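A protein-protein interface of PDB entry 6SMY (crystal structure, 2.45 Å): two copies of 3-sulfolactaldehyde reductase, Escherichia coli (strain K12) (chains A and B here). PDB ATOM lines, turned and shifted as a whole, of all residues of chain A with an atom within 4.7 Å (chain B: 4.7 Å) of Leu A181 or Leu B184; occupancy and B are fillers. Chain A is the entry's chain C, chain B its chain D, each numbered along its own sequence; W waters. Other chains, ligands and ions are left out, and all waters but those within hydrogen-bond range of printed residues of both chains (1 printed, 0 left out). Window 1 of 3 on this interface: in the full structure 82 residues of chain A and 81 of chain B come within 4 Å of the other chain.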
ATOM      1  N   TYR A 176      -1.857 -18.364   5.578  1.00  0.00           N
ATOM      2  CA  TYR A 176      -1.936 -19.832   5.679  1.00  0.00           C
ATOM      3  C   TYR A 176      -3.163 -20.297   4.902  1.00  0.00           C
ATOM      4  O   TYR A 176      -3.033 -21.117   3.952  1.00  0.00           O
ATOM      5  CB  TYR A 176      -2.046 -20.328   7.117  1.00  0.00           C
ATOM      6  CG  TYR A 176      -2.201 -21.821   7.119  1.00  0.00           C
ATOM      7  CD1 TYR A 176      -1.261 -22.612   6.475  1.00  0.00           C
ATOM      8  CD2 TYR A 176      -3.304 -22.431   7.677  1.00  0.00           C
ATOM      9  CE1 TYR A 176      -1.383 -23.984   6.437  1.00  0.00           C
ATOM     10  CE2 TYR A 176      -3.428 -23.811   7.672  1.00  0.00           C
ATOM     11  CZ  TYR A 176      -2.473 -24.587   7.032  1.00  0.00           C
ATOM     12  OH  TYR A 176      -2.588 -25.938   6.992  1.00  0.00           O
ATOM     13  N   MET A 177      -4.321 -19.760   5.294  1.00  0.00           N
ATOM     14  CA  MET A 177      -5.614 -20.148   4.701  1.00  0.00           C
ATOM     15  C   MET A 177      -5.552 -19.978   3.175  1.00  0.00           C
ATOM     16  O   MET A 177      -5.876 -20.951   2.452  1.00  0.00           O
ATOM     17  CB  MET A 177      -6.761 -19.307   5.264  1.00  0.00           C
ATOM     18  CG  MET A 177      -8.130 -19.785   4.831  1.00  0.00           C
ATOM     19  SD  MET A 177      -8.398 -21.484   5.349  1.00  0.00           S
ATOM     20  CE  MET A 177      -9.623 -22.022   4.175  1.00  0.00           C
ATOM     21  N   SER A 178      -5.167 -18.799   2.686  1.00  0.00           N
ATOM     22  CA  SER A 178      -5.282 -18.480   1.237  1.00  0.00           C
ATOM     23  C   SER A 178      -4.270 -19.316   0.442  1.00  0.00           C
ATOM     24  O   SER A 178      -4.627 -19.769  -0.647  1.00  0.00           O
ATOM     25  CB  SER A 178      -5.117 -17.021   0.954  1.00  0.00           C
ATOM     26  OG  SER A 178      -3.808 -16.600   1.317  1.00  0.00           O
ATOM     27  N   ILE A 179      -3.064 -19.527   0.974  1.00  0.00           N
ATOM     28  CA  ILE A 179      -1.983 -20.213   0.221  1.00  0.00           C
ATOM     29  C   ILE A 179      -2.350 -21.697   0.100  1.00  0.00           C
ATOM     30  O   ILE A 179      -2.257 -22.249  -1.040  1.00  0.00           O
ATOM     31  CB  ILE A 179      -0.598 -19.970   0.863  1.00  0.00           C
ATOM     32  CG1 ILE A 179      -0.234 -18.484   0.816  1.00  0.00           C
ATOM     33  CG2 ILE A 179       0.476 -20.819   0.193  1.00  0.00           C
ATOM     34  CD1 ILE A 179       0.829 -18.086   1.790  1.00  0.00           C
ATOM     35  N   ALA A 180      -2.771 -22.327   1.196  1.00  0.00           N
ATOM     36  CA  ALA A 180      -3.156 -23.754   1.215  1.00  0.00           C
ATOM     37  C   ALA A 180      -4.418 -23.946   0.380  1.00  0.00           C
ATOM     38  O   ALA A 180      -4.480 -24.941  -0.344  1.00  0.00           O
ATOM     39  CB  ALA A 180      -3.361 -24.236   2.628  1.00  0.00           C
ATOM     40  N   LEU A 181      -5.382 -23.030   0.491  1.00  0.00           N
ATOM     41  CA  LEU A 181      -6.666 -23.101  -0.260  1.00  0.00           C
ATOM     42  C   LEU A 181      -6.373 -23.151  -1.765  1.00  0.00           C
ATOM     43  O   LEU A 181      -7.100 -23.857  -2.501  1.00  0.00           O
ATOM     44  CB  LEU A 181      -7.546 -21.890   0.076  1.00  0.00           C
ATOM     45  CG  LEU A 181      -8.863 -21.799  -0.705  1.00  0.00           C
ATOM     46  CD1 LEU A 181      -9.671 -23.081  -0.625  1.00  0.00           C
ATOM     47  CD2 LEU A 181      -9.700 -20.632  -0.218  1.00  0.00           C
ATOM     48  N   ASN A 182      -5.369 -22.405  -2.204  1.00  0.00           N
ATOM     49  CA  ASN A 182      -4.988 -22.355  -3.633  1.00  0.00           C
ATOM     50  C   ASN A 182      -4.655 -23.794  -4.085  1.00  0.00           C
ATOM     51  O   ASN A 182      -5.171 -24.238  -5.122  1.00  0.00           O
ATOM     52  CB  ASN A 182      -3.876 -21.321  -3.832  1.00  0.00           C
ATOM     53  CG  ASN A 182      -3.476 -21.126  -5.279  1.00  0.00           C
ATOM     54  OD1 ASN A 182      -4.338 -21.057  -6.154  1.00  0.00           O
ATOM     55  ND2 ASN A 182      -2.174 -21.038  -5.524  1.00  0.00           N
ATOM     56  N   ALA A 183      -3.892 -24.529  -3.279  1.00  0.00           N
ATOM     57  CA  ALA A 183      -3.465 -25.920  -3.538  1.00  0.00           C
ATOM     58  C   ALA A 183      -4.685 -26.836  -3.599  1.00  0.00           C
ATOM     59  O   ALA A 183      -4.784 -27.684  -4.524  1.00  0.00           O
ATOM     60  CB  ALA A 183      -2.484 -26.360  -2.480  1.00  0.00           C
ATOM     61  N   LEU A 184      -5.606 -26.674  -2.658  1.00  0.00           N
ATOM     62  CA  LEU A 184      -6.838 -27.497  -2.608  1.00  0.00           C
ATOM     63  C   LEU A 184      -7.687 -27.178  -3.829  1.00  0.00           C
ATOM     64  O   LEU A 184      -8.175 -28.124  -4.477  1.00  0.00           O
ATOM     65  CB  LEU A 184      -7.609 -27.209  -1.318  1.00  0.00           C
ATOM     66  CG  LEU A 184      -8.926 -27.962  -1.189  1.00  0.00           C
ATOM     67  CD1 LEU A 184      -8.654 -29.457  -1.243  1.00  0.00           C
ATOM     68  CD2 LEU A 184      -9.644 -27.561   0.102  1.00  0.00           C
ATOM     69  N   SER A 185      -7.869 -25.896  -4.125  1.00  0.00           N
ATOM     70  CA  SER A 185      -8.686 -25.430  -5.276  1.00  0.00           C
ATOM     71  C   SER A 185      -8.154 -26.068  -6.562  1.00  0.00           C
ATOM     72  O   SER A 185      -8.971 -26.481  -7.407  1.00  0.00           O
ATOM     73  CB  SER A 185      -8.711 -23.924  -5.357  1.00  0.00           C
ATOM     74  OG  SER A 185      -9.193 -23.375  -4.144  1.00  0.00           O
ATOM     75  N   MET B 177     -14.487 -30.583  -2.702  1.00  0.00           N
ATOM     76  CA  MET B 177     -13.974 -29.239  -2.376  1.00  0.00           C
ATOM     77  C   MET B 177     -14.458 -28.856  -0.972  1.00  0.00           C
ATOM     78  O   MET B 177     -13.599 -28.456  -0.132  1.00  0.00           O
ATOM     79  CB  MET B 177     -14.435 -28.215  -3.411  1.00  0.00           C
ATOM     80  CG  MET B 177     -13.837 -26.846  -3.226  1.00  0.00           C
ATOM     81  SD  MET B 177     -12.048 -26.911  -3.325  1.00  0.00           S
ATOM     82  CE  MET B 177     -11.598 -25.408  -2.471  1.00  0.00           C
ATOM     83  N   ALA B 180     -12.992 -31.266   2.085  1.00  0.00           N
ATOM     84  CA  ALA B 180     -11.550 -31.016   2.315  1.00  0.00           C
ATOM     85  C   ALA B 180     -11.356 -29.611   2.884  1.00  0.00           C
ATOM     86  O   ALA B 180     -10.536 -29.459   3.819  1.00  0.00           O
ATOM     87  CB  ALA B 180     -10.774 -31.216   1.039  1.00  0.00           C
ATOM     88  N   LEU B 181     -12.068 -28.623   2.339  1.00  0.00           N
ATOM     89  CA  LEU B 181     -11.990 -27.197   2.778  1.00  0.00           C
ATOM     90  C   LEU B 181     -12.300 -27.114   4.275  1.00  0.00           C
ATOM     91  O   LEU B 181     -11.678 -26.283   4.979  1.00  0.00           O
ATOM     92  CB  LEU B 181     -12.971 -26.335   1.971  1.00  0.00           C
ATOM     93  CG  LEU B 181     -13.069 -24.864   2.383  1.00  0.00           C
ATOM     94  CD1 LEU B 181     -11.716 -24.182   2.430  1.00  0.00           C
ATOM     95  CD2 LEU B 181     -13.986 -24.066   1.469  1.00  0.00           C
ATOM     96  N   ASN B 182     -13.248 -27.930   4.737  1.00  0.00           N
ATOM     97  CA  ASN B 182     -13.669 -27.947   6.163  1.00  0.00           C
ATOM     98  C   ASN B 182     -12.421 -28.245   7.008  1.00  0.00           C
ATOM     99  O   ASN B 182     -12.162 -27.515   7.980  1.00  0.00           O
ATOM    100  CB  ASN B 182     -14.853 -28.907   6.354  1.00  0.00           C
ATOM    101  CG  ASN B 182     -15.395 -28.955   7.765  1.00  0.00           C
ATOM    102  OD1 ASN B 182     -15.543 -27.919   8.420  1.00  0.00           O
ATOM    103  ND2 ASN B 182     -15.666 -30.168   8.242  1.00  0.00           N
ATOM    104  N   ALA B 183     -11.642 -29.251   6.610  1.00  0.00           N
ATOM    105  CA  ALA B 183     -10.421 -29.693   7.322  1.00  0.00           C
ATOM    106  C   ALA B 183      -9.380 -28.560   7.317  1.00  0.00           C
ATOM    107  O   ALA B 183      -8.749 -28.298   8.363  1.00  0.00           O
ATOM    108  CB  ALA B 183      -9.891 -30.937   6.640  1.00  0.00           C
ATOM    109  N   LEU B 184      -9.199 -27.900   6.173  1.00  0.00           N
ATOM    110  CA  LEU B 184      -8.225 -26.793   6.071  1.00  0.00           C
ATOM    111  C   LEU B 184      -8.693 -25.636   6.961  1.00  0.00           C
ATOM    112  O   LEU B 184      -7.863 -25.075   7.716  1.00  0.00           O
ATOM    113  CB  LEU B 184      -8.087 -26.340   4.619  1.00  0.00           C
ATOM    114  CG  LEU B 184      -7.124 -25.165   4.441  1.00  0.00           C
ATOM    115  CD1 LEU B 184      -5.750 -25.547   4.933  1.00  0.00           C
ATOM    116  CD2 LEU B 184      -7.053 -24.689   2.992  1.00  0.00           C
ATOM    117  N   SER B 185      -9.968 -25.280   6.864  1.00  0.00           N
ATOM    118  CA  SER B 185     -10.565 -24.166   7.647  1.00  0.00           C
ATOM    119  C   SER B 185     -10.318 -24.409   9.139  1.00  0.00           C
ATOM    120  O   SER B 185      -9.979 -23.431   9.862  1.00  0.00           O
ATOM    121  CB  SER B 185     -12.032 -24.007   7.339  1.00  0.00           C
ATOM    122  OG  SER B 185     -12.238 -23.847   5.936  1.00  0.00           O
ATOM    123  N   ALA B 186     -10.434 -25.671   9.571  1.00  0.00           N
ATOM    124  CA  ALA B 186     -10.206 -26.087  10.968  1.00  0.00           C
ATOM    125  C   ALA B 186      -8.763 -25.777  11.371  1.00  0.00           C
ATOM    126  O   ALA B 186      -8.561 -25.193  12.457  1.00  0.00           O
ATOM    127  CB  ALA B 186     -10.537 -27.546  11.148  1.00  0.00           C
ATOM    128  N   GLU B 187      -7.788 -26.125  10.529  1.00  0.00           N
ATOM    129  CA  GLU B 187      -6.351 -25.893  10.838  1.00  0.00           C
ATOM    130  C   GLU B 187      -6.122 -24.394  11.071  1.00  0.00           C
ATOM    131  O   GLU B 187      -5.482 -24.030  12.069  1.00  0.00           O
ATOM    132  CB  GLU B 187      -5.469 -26.409   9.703  1.00  0.00           C
ATOM    133  CG  GLU B 187      -5.512 -27.907   9.587  1.00  0.00           C
ATOM    134  CD  GLU B 187      -4.629 -28.496   8.506  1.00  0.00           C
ATOM    135  OE1 GLU B 187      -3.875 -27.730   7.855  1.00  0.00           O
ATOM    136  OE2 GLU B 187      -4.718 -29.712   8.308  1.00  0.00           O
ATOM    137  N   ALA B 188      -6.635 -23.562  10.166  1.00  0.00           N
ATOM    138  CA  ALA B 188      -6.458 -22.098  10.213  1.00  0.00           C
ATOM    139  C   ALA B 188      -7.088 -21.576  11.507  1.00  0.00           C
ATOM    140  O   ALA B 188      -6.434 -20.768  12.195  1.00  0.00           O
ATOM    141  CB  ALA B 188      -7.052 -21.450   8.993  1.00  0.00           C
ATOM    142  N   ALA B 210      -8.655 -13.906  -0.772  1.00  0.00           N
ATOM    143  CA  ALA B 210      -8.921 -15.240  -1.353  1.00  0.00           C
ATOM    144  C   ALA B 210      -9.108 -16.279  -0.227  1.00  0.00           C
ATOM    145  O   ALA B 210      -9.759 -17.305  -0.498  1.00  0.00           O
ATOM    146  CB  ALA B 210      -7.800 -15.632  -2.285  1.00  0.00           C
ATOM    147  N   ALA B 211      -8.587 -16.032   0.977  1.00  0.00           N
ATOM    148  CA  ALA B 211      -8.773 -16.911   2.159  1.00  0.00           C
ATOM    149  C   ALA B 211     -10.262 -17.192   2.393  1.00  0.00           C
ATOM    150  O   ALA B 211     -10.612 -18.373   2.589  1.00  0.00           O
ATOM    151  CB  ALA B 211      -8.138 -16.325   3.394  1.00  0.00           C
ATOM    152  N   GLY B 214     -12.189 -17.270  -1.748  1.00  0.00           N
ATOM    153  CA  GLY B 214     -11.714 -18.337  -2.648  1.00  0.00           C
ATOM    154  C   GLY B 214     -10.896 -17.765  -3.795  1.00  0.00           C
ATOM    155  O   GLY B 214     -10.866 -16.547  -3.961  1.00  0.00           O
ATOM    156  N   HIS B 215     -10.251 -18.622  -4.568  1.00  0.00           N
ATOM    157  CA  HIS B 215      -9.360 -18.245  -5.696  1.00  0.00           C
ATOM    158  C   HIS B 215     -10.095 -18.369  -7.020  1.00  0.00           C
ATOM    159  O   HIS B 215      -9.688 -17.647  -7.945  1.00  0.00           O
ATOM    160  CB  HIS B 215      -8.124 -19.136  -5.724  1.00  0.00           C
ATOM    161  CG  HIS B 215      -7.193 -18.930  -4.594  1.00  0.00           C
ATOM    162  ND1 HIS B 215      -6.159 -18.045  -4.665  1.00  0.00           N
ATOM    163  CD2 HIS B 215      -7.129 -19.535  -3.391  1.00  0.00           C
ATOM    164  CE1 HIS B 215      -5.476 -18.114  -3.538  1.00  0.00           C
ATOM    165  NE2 HIS B 215      -6.039 -19.032  -2.748  1.00  0.00           N
ATOM    166  N   LEU B 258      -2.851 -30.624   6.291  1.00  0.00           N
ATOM    167  CA  LEU B 258      -3.142 -30.041   4.955  1.00  0.00           C
ATOM    168  C   LEU B 258      -2.095 -28.973   4.625  1.00  0.00           C
ATOM    169  O   LEU B 258      -1.593 -28.965   3.496  1.00  0.00           O
ATOM    170  CB  LEU B 258      -4.569 -29.481   4.884  1.00  0.00           C
ATOM    171  CG  LEU B 258      -5.621 -30.528   4.524  1.00  0.00           C
ATOM    172  CD1 LEU B 258      -5.872 -31.449   5.699  1.00  0.00           C
ATOM    173  CD2 LEU B 258      -6.912 -29.898   4.028  1.00  0.00           C
HETATM  174  O   HOH W   1     -10.918 -21.360  -4.143  1.00  0.00           O
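Hydrophobic or aromatic side chains of chain B within 4 Å of the printed part of chain A: Met B177, Ala B180, Leu B181, Leu B184, Ala B188, Ala B211 and His B215. Along chain B the printed residues that touch a printed residue of chain A span positions 177 to 258. Among the printed residues, 23 pairs touch across the chains. Among the printed residues, no Asp or Glu carboxylate lies within 4 Å of a Lys or Arg side-chain nitrogen of the other chain.
Water W1 lies within hydrogen-bond range of OG of Ser A185 (2.7 Å) and N of His B215 (2.8 Å).
Met A177 touches Leu B181, and with the chains exchanged Leu A181 touches Met B177. Met A177 touches Ser B185, and with the chains exchanged Ser A185 touches Met B177. Leu A181 touches its own counterpart, Leu B181. Leu A181 touches Leu B184, and with the chains exchanged Leu A184 touches Leu B181. Positions printed for both chains: 177, 180, 181, 182, 183, 184 and 185. Of the 23 pairs that touch across the chains among the printed residues, 11 have their exchanged pair printed and touching as well.
The backbone carbonyl oxygen (O) of Ser A178 lies within hydrogen-bond range of a ring nitrogen (NE2) of His B215, 2.6 Å away. N of Asn A182 sits close to NE2 of His B215 (3.5 Å). The side-chain hydroxyl (OH) of Tyr A176 lies close to the side-chain carboxylate (OE1) of Glu B187, at 2.4 Å.
OG of Ser A185 sits at hydrogen-bond distance from O of Leu A181 (2.7 Å). The side-chain hydroxyl of Ser B185 lies within hydrogen-bond range of the backbone carbonyl oxygen of Leu B181, at 2.7 Å. OE2 of Glu B187 sits at hydrogen-bond distance from N of Leu B258, at 2.9 Å.
Printed residues of chain B within 4 Å of Leu A181: Met B177 (3.5 Å), Leu B181 (3.8 Å), Leu B184 (3.4 Å), Ala B210 (3.3 Å), Ala B211 (3.7 Å), Gly B214 (3.9 Å) and His B215 (3.9 Å). Of the printed residues of chain B, Asn A182 touches His B215. Of the printed residues of chain A, Leu B181 touches Met A177 (3.5 Å), Leu A181 (3.8 Å) and Leu A184 (3.5 Å). Of the printed residues of chain A, Leu B184 touches Tyr A176, Met A177, Ala A180 and Leu A181. Of the printed residues of chain A, Glu B187 touches Tyr A176 (2.4 Å). Of the printed residues of chain A, His B215 touches Ser A178, Leu A181 and Asn A182. The nearest printed residue of chain A that does not touch Leu B184 is Leu A184 (4.8 Å). The nearest printed residue of chain A that does not touch His B215 is Ser A185 (4.4 Å).
Leu B258 touches Tyr A176 (C to OH, 3.9 Å). CE of Met A177 touches CD1 of Leu B181, 3.5 Å away. Met A177 touches Leu B184. CG of Met A177 touches O of Ala B211 (3.6 Å). Leu B184 touches Ala A180. N of Leu A181 touches CD2 of Leu B184, 3.4 Å away. Ala B211 touches Leu A181 (O to CD2, 3.7 Å). Leu A181 touches Gly B214. Leu A184 touches Ala B180 (CD1 to CB, 3.6 Å). OG of Ser A185 touches CE of Met B177, at 3.6 Å.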
